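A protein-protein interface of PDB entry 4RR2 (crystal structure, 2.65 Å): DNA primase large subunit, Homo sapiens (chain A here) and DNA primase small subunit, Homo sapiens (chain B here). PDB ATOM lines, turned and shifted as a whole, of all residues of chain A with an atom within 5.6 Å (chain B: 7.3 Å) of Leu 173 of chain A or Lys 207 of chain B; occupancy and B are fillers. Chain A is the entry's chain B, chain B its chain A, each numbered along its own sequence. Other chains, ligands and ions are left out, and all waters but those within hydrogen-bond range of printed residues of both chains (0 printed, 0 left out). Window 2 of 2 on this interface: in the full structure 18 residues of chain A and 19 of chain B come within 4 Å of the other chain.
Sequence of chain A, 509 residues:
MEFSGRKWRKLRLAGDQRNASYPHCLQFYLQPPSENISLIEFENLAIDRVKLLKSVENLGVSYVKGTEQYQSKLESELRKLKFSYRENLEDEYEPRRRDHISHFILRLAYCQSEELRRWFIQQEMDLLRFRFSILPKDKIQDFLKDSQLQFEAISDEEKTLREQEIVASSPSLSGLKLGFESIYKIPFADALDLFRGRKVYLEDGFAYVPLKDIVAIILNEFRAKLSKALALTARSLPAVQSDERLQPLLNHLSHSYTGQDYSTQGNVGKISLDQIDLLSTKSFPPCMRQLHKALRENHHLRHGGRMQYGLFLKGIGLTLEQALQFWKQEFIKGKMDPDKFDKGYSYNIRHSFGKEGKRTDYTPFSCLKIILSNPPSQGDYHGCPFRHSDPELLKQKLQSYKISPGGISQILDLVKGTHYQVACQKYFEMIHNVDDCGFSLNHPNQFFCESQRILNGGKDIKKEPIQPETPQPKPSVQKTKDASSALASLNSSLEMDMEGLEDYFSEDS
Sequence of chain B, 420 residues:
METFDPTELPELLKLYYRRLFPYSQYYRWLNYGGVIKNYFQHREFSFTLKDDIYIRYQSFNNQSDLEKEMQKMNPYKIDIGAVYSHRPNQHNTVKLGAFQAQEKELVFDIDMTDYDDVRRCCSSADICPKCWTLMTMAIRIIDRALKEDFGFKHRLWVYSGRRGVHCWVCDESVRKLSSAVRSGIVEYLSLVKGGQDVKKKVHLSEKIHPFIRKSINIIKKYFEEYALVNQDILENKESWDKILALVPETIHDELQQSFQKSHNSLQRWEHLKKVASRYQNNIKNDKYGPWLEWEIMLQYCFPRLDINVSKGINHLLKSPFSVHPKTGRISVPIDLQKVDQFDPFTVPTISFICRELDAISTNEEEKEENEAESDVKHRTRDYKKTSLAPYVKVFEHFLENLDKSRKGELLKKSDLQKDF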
ATOM      1  N   ILE A 166      -5.106  16.097  21.887  1.00  0.00           N
ATOM      2  CA  ILE A 166      -5.557  14.739  22.118  1.00  0.00           C
ATOM      3  C   ILE A 166      -7.065  14.641  22.214  1.00  0.00           C
ATOM      4  O   ILE A 166      -7.688  13.843  21.525  1.00  0.00           O
ATOM      5  CB  ILE A 166      -4.919  14.175  23.384  1.00  0.00           C
ATOM      6  CG1 ILE A 166      -3.430  13.933  23.124  1.00  0.00           C
ATOM      7  CG2 ILE A 166      -5.626  12.904  23.794  1.00  0.00           C
ATOM      8  CD1 ILE A 166      -2.649  13.467  24.321  1.00  0.00           C
ATOM      9  N   VAL A 167      -7.660  15.467  23.058  1.00  0.00           N
ATOM     10  CA  VAL A 167      -9.105  15.438  23.209  1.00  0.00           C
ATOM     11  C   VAL A 167      -9.844  15.683  21.901  1.00  0.00           C
ATOM     12  O   VAL A 167     -10.959  15.203  21.710  1.00  0.00           O
ATOM     13  CB  VAL A 167      -9.565  16.485  24.224  1.00  0.00           C
ATOM     14  CG1 VAL A 167     -11.095  16.455  24.362  1.00  0.00           C
ATOM     15  CG2 VAL A 167      -8.891  16.220  25.553  1.00  0.00           C
ATOM     16  N   ALA A 168      -9.218  16.428  21.000  1.00  0.00           N
ATOM     17  CA  ALA A 168      -9.843  16.757  19.724  1.00  0.00           C
ATOM     18  C   ALA A 168      -9.631  15.688  18.662  1.00  0.00           C
ATOM     19  O   ALA A 168     -10.429  15.557  17.733  1.00  0.00           O
ATOM     20  CB  ALA A 168      -9.315  18.088  19.232  1.00  0.00           C
ATOM     21  N   SER A 169      -8.549  14.928  18.804  1.00  0.00           N
ATOM     22  CA  SER A 169      -8.218  13.865  17.860  1.00  0.00           C
ATOM     23  C   SER A 169      -9.151  12.659  18.046  1.00  0.00           C
ATOM     24  O   SER A 169      -9.608  12.048  17.077  1.00  0.00           O
ATOM     25  CB  SER A 169      -6.762  13.421  18.066  1.00  0.00           C
ATOM     26  OG  SER A 169      -5.872  14.527  18.136  1.00  0.00           O
ATOM     27  N   SER A 170      -9.430  12.340  19.304  1.00  0.00           N
ATOM     28  CA  SER A 170     -10.280  11.219  19.693  1.00  0.00           C
ATOM     29  C   SER A 170     -11.572  11.016  18.911  1.00  0.00           C
ATOM     30  O   SER A 170     -11.938  11.827  18.065  1.00  0.00           O
ATOM     31  CB  SER A 170     -10.615  11.363  21.167  1.00  0.00           C
ATOM     32  OG  SER A 170      -9.421  11.559  21.892  1.00  0.00           O
ATOM     33  N   PRO A 171     -12.283   9.911  19.190  1.00  0.00           N
ATOM     34  CA  PRO A 171     -13.540   9.641  18.487  1.00  0.00           C
ATOM     35  C   PRO A 171     -14.578  10.683  18.890  1.00  0.00           C
ATOM     36  O   PRO A 171     -14.227  11.822  19.213  1.00  0.00           O
ATOM     37  CB  PRO A 171     -13.905   8.239  18.975  1.00  0.00           C
ATOM     38  CG  PRO A 171     -13.360   8.224  20.382  1.00  0.00           C
ATOM     39  CD  PRO A 171     -11.997   8.846  20.174  1.00  0.00           C
ATOM     40  N   SER A 172     -15.854  10.294  18.865  1.00  0.00           N
ATOM     41  CA  SER A 172     -16.928  11.197  19.268  1.00  0.00           C
ATOM     42  C   SER A 172     -16.831  11.292  20.796  1.00  0.00           C
ATOM     43  O   SER A 172     -17.632  11.977  21.445  1.00  0.00           O
ATOM     44  CB  SER A 172     -18.297  10.636  18.845  1.00  0.00           C
ATOM     45  OG  SER A 172     -19.350  11.552  19.115  1.00  0.00           O
ATOM     46  N   LEU A 173     -15.836  10.584  21.340  1.00  0.00           N
ATOM     47  CA  LEU A 173     -15.521  10.528  22.772  1.00  0.00           C
ATOM     48  C   LEU A 173     -15.974  11.793  23.500  1.00  0.00           C
ATOM     49  O   LEU A 173     -15.199  12.735  23.690  1.00  0.00           O
ATOM     50  CB  LEU A 173     -14.008  10.314  22.933  1.00  0.00           C
ATOM     51  CG  LEU A 173     -13.281  10.299  24.277  1.00  0.00           C
ATOM     52  CD1 LEU A 173     -12.013   9.444  24.138  1.00  0.00           C
ATOM     53  CD2 LEU A 173     -12.933  11.718  24.717  1.00  0.00           C
ATOM     54  N   SER A 174     -17.246  11.798  23.900  1.00  0.00           N
ATOM     55  CA  SER A 174     -17.848  12.936  24.587  1.00  0.00           C
ATOM     56  C   SER A 174     -16.986  13.386  25.761  1.00  0.00           C
ATOM     57  O   SER A 174     -16.182  12.615  26.288  1.00  0.00           O
ATOM     58  CB  SER A 174     -19.256  12.572  25.068  1.00  0.00           C
ATOM     59  OG  SER A 174     -19.941  13.718  25.545  1.00  0.00           O
ATOM     60  N   GLY A 175     -17.152  14.641  26.163  1.00  0.00           N
ATOM     61  CA  GLY A 175     -16.361  15.168  27.258  1.00  0.00           C
ATOM     62  C   GLY A 175     -15.172  15.960  26.741  1.00  0.00           C
ATOM     63  O   GLY A 175     -14.823  15.887  25.561  1.00  0.00           O
ATOM     64  N   LYS A 177     -12.408  16.165  29.007  1.00  0.00           N
ATOM     65  CA  LYS A 177     -11.440  15.785  30.033  1.00  0.00           C
ATOM     66  C   LYS A 177     -10.561  14.638  29.572  1.00  0.00           C
ATOM     67  O   LYS A 177     -11.064  13.605  29.120  1.00  0.00           O
ATOM     68  CB  LYS A 177     -12.157  15.351  31.315  1.00  0.00           C
ATOM     69  CG  LYS A 177     -12.962  16.444  31.980  1.00  0.00           C
ATOM     70  CD  LYS A 177     -13.680  15.933  33.217  1.00  0.00           C
ATOM     71  CE  LYS A 177     -14.482  17.053  33.869  1.00  0.00           C
ATOM     72  NZ  LYS A 177     -15.217  16.577  35.070  1.00  0.00           N
ATOM     73  N   LEU B 204     -17.916  18.285   8.461  1.00  0.00           N
ATOM     74  CA  LEU B 204     -17.146  18.312   9.679  1.00  0.00           C
ATOM     75  C   LEU B 204     -18.099  17.854  10.749  1.00  0.00           C
ATOM     76  O   LEU B 204     -19.315  17.964  10.593  1.00  0.00           O
ATOM     77  CB  LEU B 204     -16.649  19.725   9.968  1.00  0.00           C
ATOM     78  CG  LEU B 204     -15.697  20.254   8.905  1.00  0.00           C
ATOM     79  CD1 LEU B 204     -15.297  21.661   9.250  1.00  0.00           C
ATOM     80  CD2 LEU B 204     -14.479  19.369   8.828  1.00  0.00           C
ATOM     81  N   SER B 205     -17.546  17.303  11.816  1.00  0.00           N
ATOM     82  CA  SER B 205     -18.358  16.837  12.919  1.00  0.00           C
ATOM     83  C   SER B 205     -18.098  17.858  14.008  1.00  0.00           C
ATOM     84  O   SER B 205     -17.117  18.583  13.926  1.00  0.00           O
ATOM     85  CB  SER B 205     -17.904  15.441  13.352  1.00  0.00           C
ATOM     86  OG  SER B 205     -16.584  15.468  13.870  1.00  0.00           O
ATOM     87  N   GLU B 206     -18.963  17.935  15.012  1.00  0.00           N
ATOM     88  CA  GLU B 206     -18.769  18.910  16.079  1.00  0.00           C
ATOM     89  C   GLU B 206     -17.283  19.010  16.424  1.00  0.00           C
ATOM     90  O   GLU B 206     -16.716  20.104  16.430  1.00  0.00           O
ATOM     91  CB  GLU B 206     -19.578  18.523  17.322  1.00  0.00           C
ATOM     92  CG  GLU B 206     -19.647  19.622  18.394  1.00  0.00           C
ATOM     93  CD  GLU B 206     -20.439  20.859  17.945  1.00  0.00           C
ATOM     94  OE1 GLU B 206     -20.404  21.891  18.666  1.00  0.00           O
ATOM     95  OE2 GLU B 206     -21.100  20.796  16.878  1.00  0.00           O
ATOM     96  N   LYS B 207     -16.653  17.867  16.692  1.00  0.00           N
ATOM     97  CA  LYS B 207     -15.227  17.820  17.025  1.00  0.00           C
ATOM     98  C   LYS B 207     -14.407  18.090  15.757  1.00  0.00           C
ATOM     99  O   LYS B 207     -14.847  17.763  14.655  1.00  0.00           O
ATOM    100  CB  LYS B 207     -14.888  16.434  17.569  1.00  0.00           C
ATOM    101  CG  LYS B 207     -14.252  16.401  18.942  1.00  0.00           C
ATOM    102  CD  LYS B 207     -14.925  15.326  19.786  1.00  0.00           C
ATOM    103  CE  LYS B 207     -14.067  14.923  20.970  1.00  0.00           C
ATOM    104  NZ  LYS B 207     -12.835  14.205  20.531  1.00  0.00           N
ATOM    105  N   ILE B 208     -13.223  18.684  15.906  1.00  0.00           N
ATOM    106  CA  ILE B 208     -12.364  18.986  14.754  1.00  0.00           C
ATOM    107  C   ILE B 208     -10.919  18.529  14.976  1.00  0.00           C
ATOM    108  O   ILE B 208     -10.195  19.105  15.784  1.00  0.00           O
ATOM    109  CB  ILE B 208     -12.351  20.509  14.425  1.00  0.00           C
ATOM    110  CG1 ILE B 208     -13.684  20.935  13.811  1.00  0.00           C
ATOM    111  CG2 ILE B 208     -11.242  20.825  13.448  1.00  0.00           C
ATOM    112  CD1 ILE B 208     -14.032  20.181  12.552  1.00  0.00           C
ATOM    113  N   HIS B 209     -10.494  17.501  14.247  1.00  0.00           N
ATOM    114  CA  HIS B 209      -9.137  16.997  14.402  1.00  0.00           C
ATOM    115  C   HIS B 209      -8.141  18.121  14.117  1.00  0.00           C
ATOM    116  O   HIS B 209      -8.309  18.876  13.161  1.00  0.00           O
ATOM    117  CB  HIS B 209      -8.897  15.817  13.440  1.00  0.00           C
ATOM    118  CG  HIS B 209      -7.598  15.111  13.667  1.00  0.00           C
ATOM    119  ND1 HIS B 209      -6.377  15.694  13.402  1.00  0.00           N
ATOM    120  CD2 HIS B 209      -7.324  13.895  14.194  1.00  0.00           C
ATOM    121  CE1 HIS B 209      -5.408  14.873  13.759  1.00  0.00           C
ATOM    122  NE2 HIS B 209      -5.957  13.773  14.244  1.00  0.00           N
ATOM    123  N   ILE B 212      -7.113  19.040  10.601  1.00  0.00           N
ATOM    124  CA  ILE B 212      -8.114  19.782   9.871  1.00  0.00           C
ATOM    125  C   ILE B 212      -8.070  21.236  10.285  1.00  0.00           C
ATOM    126  O   ILE B 212      -8.147  22.124   9.445  1.00  0.00           O
ATOM    127  CB  ILE B 212      -9.527  19.267  10.144  1.00  0.00           C
ATOM    128  CG1 ILE B 212      -9.724  17.913   9.481  1.00  0.00           C
ATOM    129  CG2 ILE B 212     -10.543  20.245   9.599  1.00  0.00           C
ATOM    130  CD1 ILE B 212     -11.135  17.404   9.598  1.00  0.00           C
ATOM    131  N   TRP B 291     -20.069  25.273  11.630  1.00  0.00           N
ATOM    132  CA  TRP B 291     -18.985  24.721  10.832  1.00  0.00           C
ATOM    133  C   TRP B 291     -19.239  24.907   9.340  1.00  0.00           C
ATOM    134  O   TRP B 291     -18.324  24.794   8.534  1.00  0.00           O
ATOM    135  CB  TRP B 291     -18.821  23.236  11.150  1.00  0.00           C
ATOM    136  CG  TRP B 291     -18.152  22.923  12.470  1.00  0.00           C
ATOM    137  CD1 TRP B 291     -17.886  21.681  12.961  1.00  0.00           C
ATOM    138  CD2 TRP B 291     -17.627  23.853  13.432  1.00  0.00           C
ATOM    139  NE1 TRP B 291     -17.225  21.769  14.158  1.00  0.00           N
ATOM    140  CE2 TRP B 291     -17.048  23.089  14.475  1.00  0.00           C
ATOM    141  CE3 TRP B 291     -17.580  25.254  13.514  1.00  0.00           C
ATOM    142  CZ2 TRP B 291     -16.433  23.678  15.593  1.00  0.00           C
ATOM    143  CZ3 TRP B 291     -16.968  25.841  14.628  1.00  0.00           C
ATOM    144  CH2 TRP B 291     -16.400  25.048  15.651  1.00  0.00           C
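The side-chain hydroxyl (OG) of Ser 170 of chain A is in hydrogen-bond range of the backbone carbonyl oxygen (O) of Ile 166 of chain A (2.9 Å).
OG of Ser 205 of chain B sits at hydrogen-bond distance from O of Lys 207 of chain B.
Printed residues of chain B that touch a printed residue of chain A: Lys 207, Ile 208 and His 209.
Among the printed residues, no Asp or Glu carboxylate lies within 4 Å of a Lys or Arg side-chain nitrogen of the other chain.
Printed residues of chain B within 4 Å of Ala 168 of chain A: Lys 207 (3.9 Å), Ile 208 (3.7 Å) and His 209 (3.9 Å).
Printed residues of chain B within 4 Å of Ser 169 of chain A: His 209.
Printed residues of chain B within 4 Å of Pro 171 of chain A: Lys 207.
Printed residues of chain B within 4 Å of Leu 173 of chain A: Lys 207.
Leu 204 of chain B touches none of the printed residues of chain A.
Of the printed residues of chain A, His 209 of chain B touches Ala 168 and Ser 169.
The nearest printed residue of chain B that does not touch Leu 173 of chain A is Ser 205 of chain B (9.0 Å).
The nearest residue of chain A that does not touch Lys 207 of chain B is Ser 172 of chain A (4.6 Å).
The nearest printed residue of chain B that does not touch Ser 170 of chain A is His 209 of chain B (5.7 Å).
NZ of Lys 207 of chain B touches O of Ala 168 of chain A, at 3.9 Å.
Ile 208 of chain B touches Ala 168 of chain A (O to CB, 3.7 Å).
O of Ala 168 of chain A touches CA of His 209 of chain B, at 3.9 Å.
Ser 169 of chain A touches His 209 of chain B (CA to CD2, 3.8 Å).
Ser 170 of chain A touches Lys 207 of chain B.
Lys 207 of chain B touches Leu 173 of chain A.
The side-chain amino group (NZ) of Lys 207 of chain B sits at hydrogen-bond distance from the backbone carbonyl oxygen (O) of Val 167 of chain A (2.4 Å).
The side-chain amino group (NZ) of Lys 207 of chain B is in hydrogen-bond range of the backbone carbonyl oxygen (O) of Pro 171 of chain A, 3.1 Å away.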
